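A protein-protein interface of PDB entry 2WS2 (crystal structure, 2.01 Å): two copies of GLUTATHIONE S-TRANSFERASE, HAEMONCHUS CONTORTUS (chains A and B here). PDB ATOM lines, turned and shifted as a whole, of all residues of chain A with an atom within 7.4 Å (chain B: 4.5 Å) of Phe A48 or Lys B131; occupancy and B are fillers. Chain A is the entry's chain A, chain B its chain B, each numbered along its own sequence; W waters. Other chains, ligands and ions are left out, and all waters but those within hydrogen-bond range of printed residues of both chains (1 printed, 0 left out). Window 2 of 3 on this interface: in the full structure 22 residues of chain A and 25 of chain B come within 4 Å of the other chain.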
ATOM      1  N   TRP A  39       4.948   7.637  23.792  1.00  0.00           N
ATOM      2  CA  TRP A  39       3.637   7.899  24.389  1.00  0.00           C
ATOM      3  C   TRP A  39       2.780   6.629  24.738  1.00  0.00           C
ATOM      4  O   TRP A  39       2.202   6.578  25.810  1.00  0.00           O
ATOM      5  CB  TRP A  39       2.876   8.966  23.567  1.00  0.00           C
ATOM      6  CG  TRP A  39       1.328   8.978  23.674  1.00  0.00           C
ATOM      7  CD1 TRP A  39       0.460   8.712  22.677  1.00  0.00           C
ATOM      8  CD2 TRP A  39       0.525   9.273  24.837  1.00  0.00           C
ATOM      9  NE1 TRP A  39      -0.842   8.819  23.123  1.00  0.00           N
ATOM     10  CE2 TRP A  39      -0.833   9.149  24.448  1.00  0.00           C
ATOM     11  CE3 TRP A  39       0.817   9.596  26.165  1.00  0.00           C
ATOM     12  CZ2 TRP A  39      -1.909   9.353  25.342  1.00  0.00           C
ATOM     13  CZ3 TRP A  39      -0.248   9.788  27.062  1.00  0.00           C
ATOM     14  CH2 TRP A  39      -1.601   9.664  26.639  1.00  0.00           C
ATOM     15  N   LYS A  43       0.435   5.922  28.093  1.00  0.00           N
ATOM     16  CA  LYS A  43      -0.949   6.194  27.753  1.00  0.00           C
ATOM     17  C   LYS A  43      -1.967   5.637  28.728  1.00  0.00           C
ATOM     18  O   LYS A  43      -2.841   6.379  29.179  1.00  0.00           O
ATOM     19  CB  LYS A  43      -1.293   5.640  26.378  1.00  0.00           C
ATOM     20  CG  LYS A  43      -2.763   5.906  26.048  1.00  0.00           C
ATOM     21  CD  LYS A  43      -3.306   4.996  24.933  1.00  0.00           C
ATOM     22  CE  LYS A  43      -4.236   5.772  24.012  1.00  0.00           C
ATOM     23  NZ  LYS A  43      -3.973   5.433  22.565  1.00  0.00           N
ATOM     24  N   ALA A  44      -1.868   4.338  29.023  1.00  0.00           N
ATOM     25  CA  ALA A  44      -2.828   3.660  29.914  1.00  0.00           C
ATOM     26  C   ALA A  44      -2.740   4.192  31.339  1.00  0.00           C
ATOM     27  O   ALA A  44      -3.694   4.048  32.133  1.00  0.00           O
ATOM     28  CB  ALA A  44      -2.592   2.138  29.885  1.00  0.00           C
ATOM     29  N   SER A  45      -1.599   4.799  31.680  1.00  0.00           N
ATOM     30  CA  SER A  45      -1.380   5.372  33.007  1.00  0.00           C
ATOM     31  C   SER A  45      -2.052   6.745  33.223  1.00  0.00           C
ATOM     32  O   SER A  45      -2.019   7.264  34.336  1.00  0.00           O
ATOM     33  CB  SER A  45       0.111   5.509  33.309  1.00  0.00           C
ATOM     34  OG  SER A  45       0.605   6.810  32.963  1.00  0.00           O
ATOM     35  N   MET A  46      -2.619   7.336  32.165  1.00  0.00           N
ATOM     36  CA  MET A  46      -3.352   8.616  32.295  1.00  0.00           C
ATOM     37  C   MET A  46      -4.853   8.361  32.489  1.00  0.00           C
ATOM     38  O   MET A  46      -5.400   7.406  31.904  1.00  0.00           O
ATOM     39  CB  MET A  46      -3.092   9.555  31.122  1.00  0.00           C
ATOM     40  CG  MET A  46      -1.567   9.866  30.826  1.00  0.00           C
ATOM     41  SD  MET A  46      -0.484  10.347  32.188  1.00  0.00           S
ATOM     42  CE  MET A  46       1.034   9.614  31.626  1.00  0.00           C
ATOM     43  N   PRO A  47      -5.503   9.177  33.352  1.00  0.00           N
ATOM     44  CA  PRO A  47      -6.921   9.318  33.600  1.00  0.00           C
ATOM     45  C   PRO A  47      -7.851   9.088  32.429  1.00  0.00           C
ATOM     46  O   PRO A  47      -8.687   8.188  32.475  1.00  0.00           O
ATOM     47  CB  PRO A  47      -7.008  10.776  34.047  1.00  0.00           C
ATOM     48  CG  PRO A  47      -5.782  10.907  34.908  1.00  0.00           C
ATOM     49  CD  PRO A  47      -4.756   9.942  34.376  1.00  0.00           C
ATOM     50  N   PHE A  48      -7.756   9.917  31.400  1.00  0.00           N
ATOM     51  CA  PHE A  48      -8.575   9.680  30.240  1.00  0.00           C
ATOM     52  C   PHE A  48      -7.718   9.290  29.025  1.00  0.00           C
ATOM     53  O   PHE A  48      -8.142   9.450  27.900  1.00  0.00           O
ATOM     54  CB  PHE A  48      -9.548  10.853  29.925  1.00  0.00           C
ATOM     55  CG  PHE A  48     -10.127  11.586  31.148  1.00  0.00           C
ATOM     56  CD1 PHE A  48     -10.744  10.894  32.217  1.00  0.00           C
ATOM     57  CD2 PHE A  48     -10.115  12.993  31.189  1.00  0.00           C
ATOM     58  CE1 PHE A  48     -11.285  11.579  33.309  1.00  0.00           C
ATOM     59  CE2 PHE A  48     -10.695  13.705  32.272  1.00  0.00           C
ATOM     60  CZ  PHE A  48     -11.272  12.993  33.340  1.00  0.00           C
ATOM     61  N   GLY A  49      -6.526   8.750  29.260  1.00  0.00           N
ATOM     62  CA  GLY A  49      -5.704   8.197  28.168  1.00  0.00           C
ATOM     63  C   GLY A  49      -5.258   9.310  27.222  1.00  0.00           C
ATOM     64  O   GLY A  49      -5.213   9.139  26.006  1.00  0.00           O
ATOM     65  N   GLN A  50      -4.964  10.452  27.834  1.00  0.00           N
ATOM     66  CA  GLN A  50      -4.850  11.723  27.191  1.00  0.00           C
ATOM     67  C   GLN A  50      -3.757  12.547  27.897  1.00  0.00           C
ATOM     68  O   GLN A  50      -3.413  12.307  29.069  1.00  0.00           O
ATOM     69  CB  GLN A  50      -6.208  12.461  27.231  1.00  0.00           C
ATOM     70  CG  GLN A  50      -7.187  12.045  26.111  1.00  0.00           C
ATOM     71  CD  GLN A  50      -8.559  12.720  26.189  1.00  0.00           C
ATOM     72  OE1 GLN A  50      -9.553  12.146  25.727  1.00  0.00           O
ATOM     73  NE2 GLN A  50      -8.621  13.957  26.749  1.00  0.00           N
ATOM     74  N   LEU A  51      -3.191  13.497  27.162  1.00  0.00           N
ATOM     75  CA  LEU A  51      -2.316  14.485  27.783  1.00  0.00           C
ATOM     76  C   LEU A  51      -2.881  15.881  27.489  1.00  0.00           C
ATOM     77  O   LEU A  51      -3.589  16.058  26.497  1.00  0.00           O
ATOM     78  CB  LEU A  51      -0.877  14.314  27.286  1.00  0.00           C
ATOM     79  CG  LEU A  51      -0.033  13.107  27.717  1.00  0.00           C
ATOM     80  CD1 LEU A  51       1.397  13.181  27.078  1.00  0.00           C
ATOM     81  CD2 LEU A  51       0.060  12.919  29.237  1.00  0.00           C
ATOM     82  N   VAL A  53      -1.363  15.967  31.606  1.00  0.00           N
ATOM     83  CA  VAL A  53      -1.764  15.516  32.922  1.00  0.00           C
ATOM     84  C   VAL A  53      -0.846  16.117  33.952  1.00  0.00           C
ATOM     85  O   VAL A  53       0.382  15.996  33.845  1.00  0.00           O
ATOM     86  CB  VAL A  53      -1.623  13.986  33.038  1.00  0.00           C
ATOM     87  CG1 VAL A  53      -1.693  13.555  34.490  1.00  0.00           C
ATOM     88  CG2 VAL A  53      -2.690  13.289  32.165  1.00  0.00           C
ATOM     89  N   LEU A  61      -4.289  15.101  37.837  1.00  0.00           N
ATOM     90  CA  LEU A  61      -5.306  15.984  37.280  1.00  0.00           C
ATOM     91  C   LEU A  61      -5.267  16.065  35.740  1.00  0.00           C
ATOM     92  O   LEU A  61      -4.286  16.567  35.137  1.00  0.00           O
ATOM     93  CB  LEU A  61      -5.307  17.369  37.983  1.00  0.00           C
ATOM     94  CG  LEU A  61      -6.436  18.347  37.599  1.00  0.00           C
ATOM     95  CD1 LEU A  61      -7.845  17.990  38.166  1.00  0.00           C
ATOM     96  CD2 LEU A  61      -6.075  19.827  38.017  1.00  0.00           C
ATOM     97  N   PRO A  62      -6.322  15.543  35.075  1.00  0.00           N
ATOM     98  CA  PRO A  62      -6.374  15.707  33.636  1.00  0.00           C
ATOM     99  C   PRO A  62      -7.006  17.011  33.115  1.00  0.00           C
ATOM    100  O   PRO A  62      -7.638  17.725  33.876  1.00  0.00           O
ATOM    101  CB  PRO A  62      -7.210  14.518  33.181  1.00  0.00           C
ATOM    102  CG  PRO A  62      -8.214  14.283  34.355  1.00  0.00           C
ATOM    103  CD  PRO A  62      -7.544  14.890  35.614  1.00  0.00           C
ATOM    104  N   GLN A  63      -6.771  17.288  31.819  1.00  0.00           N
ATOM    105  CA  GLN A  63      -7.531  18.196  30.950  1.00  0.00           C
ATOM    106  C   GLN A  63      -6.911  19.609  31.094  1.00  0.00           C
ATOM    107  O   GLN A  63      -6.748  20.084  32.204  1.00  0.00           O
ATOM    108  CB  GLN A  63      -9.056  18.190  31.236  1.00  0.00           C
ATOM    109  CG  GLN A  63      -9.912  17.081  30.532  1.00  0.00           C
ATOM    110  CD  GLN A  63     -10.317  17.407  29.081  1.00  0.00           C
ATOM    111  OE1 GLN A  63     -10.097  18.501  28.587  1.00  0.00           O
ATOM    112  NE2 GLN A  63     -10.905  16.430  28.400  1.00  0.00           N
ATOM    113  N   SER B  90     -12.436  18.797  35.164  1.00  0.00           N
ATOM    114  CA  SER B  90     -11.879  17.899  34.163  1.00  0.00           C
ATOM    115  C   SER B  90     -12.955  16.981  33.543  1.00  0.00           C
ATOM    116  O   SER B  90     -13.000  16.763  32.328  1.00  0.00           O
ATOM    117  CB  SER B  90     -10.719  17.068  34.761  1.00  0.00           C
ATOM    118  OG  SER B  90     -11.110  16.273  35.872  1.00  0.00           O
ATOM    119  N   ILE B  91     -13.856  16.470  34.373  1.00  0.00           N
ATOM    120  CA  ILE B  91     -14.825  15.485  33.867  1.00  0.00           C
ATOM    121  C   ILE B  91     -15.841  16.199  32.988  1.00  0.00           C
ATOM    122  O   ILE B  91     -16.248  15.677  31.946  1.00  0.00           O
ATOM    123  CB  ILE B  91     -15.491  14.714  35.002  1.00  0.00           C
ATOM    124  CG1 ILE B  91     -14.409  14.012  35.802  1.00  0.00           C
ATOM    125  CG2 ILE B  91     -16.463  13.686  34.453  1.00  0.00           C
ATOM    126  CD1 ILE B  91     -14.839  13.420  37.126  1.00  0.00           C
ATOM    127  N   GLN B  94     -13.951  16.742  29.752  1.00  0.00           N
ATOM    128  CA  GLN B  94     -13.976  15.471  28.994  1.00  0.00           C
ATOM    129  C   GLN B  94     -15.352  15.189  28.369  1.00  0.00           C
ATOM    130  O   GLN B  94     -15.451  14.686  27.238  1.00  0.00           O
ATOM    131  CB  GLN B  94     -13.523  14.309  29.888  1.00  0.00           C
ATOM    132  CG  GLN B  94     -13.344  12.998  29.133  1.00  0.00           C
ATOM    133  CD  GLN B  94     -12.112  13.067  28.283  1.00  0.00           C
ATOM    134  OE1 GLN B  94     -11.175  13.809  28.599  1.00  0.00           O
ATOM    135  NE2 GLN B  94     -12.088  12.306  27.212  1.00  0.00           N
ATOM    136  N   PRO B 127     -16.444   4.542  18.684  1.00  0.00           N
ATOM    137  CA  PRO B 127     -15.118   4.631  19.323  1.00  0.00           C
ATOM    138  C   PRO B 127     -15.085   5.564  20.543  1.00  0.00           C
ATOM    139  O   PRO B 127     -14.259   5.368  21.449  1.00  0.00           O
ATOM    140  CB  PRO B 127     -14.206   5.225  18.228  1.00  0.00           C
ATOM    141  CG  PRO B 127     -14.935   5.125  16.960  1.00  0.00           C
ATOM    142  CD  PRO B 127     -16.357   4.669  17.216  1.00  0.00           C
ATOM    143  N   ALA B 128     -15.972   6.561  20.543  1.00  0.00           N
ATOM    144  CA  ALA B 128     -16.024   7.632  21.572  1.00  0.00           C
ATOM    145  C   ALA B 128     -16.988   7.313  22.686  1.00  0.00           C
ATOM    146  O   ALA B 128     -16.697   7.556  23.853  1.00  0.00           O
ATOM    147  CB  ALA B 128     -16.438   8.915  20.945  1.00  0.00           C
ATOM    148  N   ARG B 129     -18.152   6.798  22.303  1.00  0.00           N
ATOM    149  CA  ARG B 129     -19.161   6.348  23.242  1.00  0.00           C
ATOM    150  C   ARG B 129     -18.471   5.304  24.091  1.00  0.00           C
ATOM    151  O   ARG B 129     -18.494   5.344  25.335  1.00  0.00           O
ATOM    152  CB  ARG B 129     -20.312   5.727  22.465  1.00  0.00           C
ATOM    153  CG  ARG B 129     -21.540   5.456  23.246  1.00  0.00           C
ATOM    154  CD  ARG B 129     -22.377   4.406  22.534  1.00  0.00           C
ATOM    155  NE  ARG B 129     -21.905   3.041  22.778  1.00  0.00           N
ATOM    156  CZ  ARG B 129     -22.621   2.082  23.370  1.00  0.00           C
ATOM    157  NH1 ARG B 129     -23.858   2.323  23.783  1.00  0.00           N
ATOM    158  NH2 ARG B 129     -22.093   0.873  23.539  1.00  0.00           N
ATOM    159  N   GLN B 130     -17.822   4.369  23.409  1.00  0.00           N
ATOM    160  CA  GLN B 130     -16.965   3.416  24.110  1.00  0.00           C
ATOM    161  C   GLN B 130     -15.905   4.100  24.988  1.00  0.00           C
ATOM    162  O   GLN B 130     -15.816   3.823  26.182  1.00  0.00           O
ATOM    163  CB  GLN B 130     -16.347   2.425  23.122  1.00  0.00           C
ATOM    164  CG  GLN B 130     -17.385   1.459  22.517  1.00  0.00           C
ATOM    165  CD  GLN B 130     -17.797   0.345  23.466  1.00  0.00           C
ATOM    166  OE1 GLN B 130     -18.717  -0.433  23.161  1.00  0.00           O
ATOM    167  NE2 GLN B 130     -17.127   0.248  24.611  1.00  0.00           N
ATOM    168  N   LYS B 131     -15.101   4.983  24.405  1.00  0.00           N
ATOM    169  CA  LYS B 131     -14.055   5.670  25.174  1.00  0.00           C
ATOM    170  C   LYS B 131     -14.665   6.291  26.454  1.00  0.00           C
ATOM    171  O   LYS B 131     -14.265   5.988  27.585  1.00  0.00           O
ATOM    172  CB  LYS B 131     -13.433   6.790  24.318  1.00  0.00           C
ATOM    173  CG  LYS B 131     -11.950   7.033  24.517  1.00  0.00           C
ATOM    174  CD  LYS B 131     -11.671   8.526  24.803  1.00  0.00           C
ATOM    175  CE  LYS B 131     -10.237   8.752  25.213  1.00  0.00           C
ATOM    176  NZ  LYS B 131      -9.445   9.279  24.046  1.00  0.00           N
ATOM    177  N   PHE B 132     -15.648   7.161  26.248  1.00  0.00           N
ATOM    178  CA  PHE B 132     -16.194   7.994  27.334  1.00  0.00           C
ATOM    179  C   PHE B 132     -17.039   7.148  28.330  1.00  0.00           C
ATOM    180  O   PHE B 132     -16.823   7.166  29.542  1.00  0.00           O
ATOM    181  CB  PHE B 132     -16.955   9.186  26.714  1.00  0.00           C
ATOM    182  CG  PHE B 132     -17.677  10.035  27.701  1.00  0.00           C
ATOM    183  CD1 PHE B 132     -16.967  10.839  28.589  1.00  0.00           C
ATOM    184  CD2 PHE B 132     -19.062  10.011  27.773  1.00  0.00           C
ATOM    185  CE1 PHE B 132     -17.618  11.629  29.499  1.00  0.00           C
ATOM    186  CE2 PHE B 132     -19.742  10.795  28.710  1.00  0.00           C
ATOM    187  CZ  PHE B 132     -19.009  11.604  29.579  1.00  0.00           C
ATOM    188  N   PHE B 133     -17.927   6.310  27.829  1.00  0.00           N
ATOM    189  CA  PHE B 133     -18.748   5.582  28.792  1.00  0.00           C
ATOM    190  C   PHE B 133     -17.914   4.629  29.629  1.00  0.00           C
ATOM    191  O   PHE B 133     -18.155   4.477  30.820  1.00  0.00           O
ATOM    192  CB  PHE B 133     -19.952   4.920  28.146  1.00  0.00           C
ATOM    193  CG  PHE B 133     -21.073   5.863  27.854  1.00  0.00           C
ATOM    194  CD1 PHE B 133     -22.107   5.480  27.013  1.00  0.00           C
ATOM    195  CD2 PHE B 133     -21.091   7.155  28.392  1.00  0.00           C
ATOM    196  CE1 PHE B 133     -23.161   6.339  26.730  1.00  0.00           C
ATOM    197  CE2 PHE B 133     -22.127   8.027  28.105  1.00  0.00           C
ATOM    198  CZ  PHE B 133     -23.164   7.625  27.274  1.00  0.00           C
ATOM    199  N   THR B 134     -16.883   4.042  29.031  1.00  0.00           N
ATOM    200  CA  THR B 134     -15.919   3.259  29.797  1.00  0.00           C
ATOM    201  C   THR B 134     -15.162   4.169  30.784  1.00  0.00           C
ATOM    202  O   THR B 134     -14.778   3.733  31.878  1.00  0.00           O
ATOM    203  CB  THR B 134     -14.930   2.489  28.873  1.00  0.00           C
ATOM    204  OG1 THR B 134     -15.653   1.774  27.859  1.00  0.00           O
ATOM    205  CG2 THR B 134     -14.081   1.504  29.648  1.00  0.00           C
ATOM    206  N   ILE B 135     -14.937   5.427  30.403  1.00  0.00           N
ATOM    207  CA  ILE B 135     -14.275   6.360  31.314  1.00  0.00           C
ATOM    208  C   ILE B 135     -15.157   6.593  32.523  1.00  0.00           C
ATOM    209  O   ILE B 135     -14.734   6.375  33.640  1.00  0.00           O
ATOM    210  CB  ILE B 135     -13.966   7.745  30.654  1.00  0.00           C
ATOM    211  CG1 ILE B 135     -12.662   7.658  29.866  1.00  0.00           C
ATOM    212  CG2 ILE B 135     -13.988   8.854  31.750  1.00  0.00           C
ATOM    213  CD1 ILE B 135     -12.540   8.613  28.670  1.00  0.00           C
ATOM    214  N   ILE B 139     -14.707   5.682  36.623  1.00  0.00           N
ATOM    215  CA  ILE B 139     -14.786   6.749  37.639  1.00  0.00           C
ATOM    216  C   ILE B 139     -15.856   6.412  38.705  1.00  0.00           C
ATOM    217  O   ILE B 139     -15.562   6.397  39.896  1.00  0.00           O
ATOM    218  CB  ILE B 139     -15.046   8.128  36.991  1.00  0.00           C
ATOM    219  CG1 ILE B 139     -13.752   8.666  36.366  1.00  0.00           C
ATOM    220  CG2 ILE B 139     -15.558   9.118  38.031  1.00  0.00           C
ATOM    221  CD1 ILE B 139     -14.006   9.900  35.482  1.00  0.00           C
HETATM  222  O   HOH W   1     -10.874  12.012  22.965  1.00  0.00           O
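No position is printed for both chains. Of the 10 pairs that touch across the chains among the printed residues, none has its exchanged pair printed and touching as well.
Water W1 lies within hydrogen-bond range of OE1 of Gln A50 (3.1 Å) and NZ of Lys B131 (3.3 Å).
O of Ser B90 touches CE2 of Phe A48, 3.8 Å away. Phe A48 touches Gln B94. CE of Lys B131 touches O of Phe A48, 3.5 Å away. Ile B135 touches Phe A48 (CG2 to CD1, 3.9 Å). CD1 of Ile B139 touches CE1 of Phe A48, 3.9 Å away. Ser B90 touches Pro A62. O of Ser B90 touches CG of Gln A63, 3.6 Å away.
OE1 of Gln A50 is in hydrogen-bond range of NE2 of Gln B94, at 2.9 Å. NZ of Lys B131 is in hydrogen-bond range of OE1 of Gln A50 (3.3 Å). NE2 of Gln A63 is in hydrogen-bond range of OE1 of Gln B94, at 2.6 Å.
Of chain B, only Ser B90, Gln B94, Lys B131, Ile B135 and Ile B139 come within 4 Å of Phe A48. Lys B131 touches just these residues of chain A: Phe A48 and Gln A50. Of the printed residues of chain A, Ile B135 touches Phe A48 (3.9 Å). Of the printed residues of chain A, Ile B139 touches Phe A48. Printed residues of chain B within 4 Å of Pro A62: Ser B90 (3.3 Å). Printed residues of chain B within 4 Å of Gln A50: Gln B94 (2.9 Å) and Lys B131 (3.3 Å). Val A53 touches none of the printed residues of chain B. The nearest residue of chain A that does not touch Lys B131 is Gly A49 (4.7 Å). The nearest printed residue of chain A that does not touch Gln B94 is Pro A62 (6.1 Å).
Of the 13 printed residues of chain B, 5 touch a printed residue of chain A. Printed residues of chain A that touch a printed residue of chain B: Phe A48, Gln A50, Pro A62 and Gln A63. Hydrophobic or aromatic side chains of chain A within 4 Å of the printed part of chain B: Phe A48 and Pro A62.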
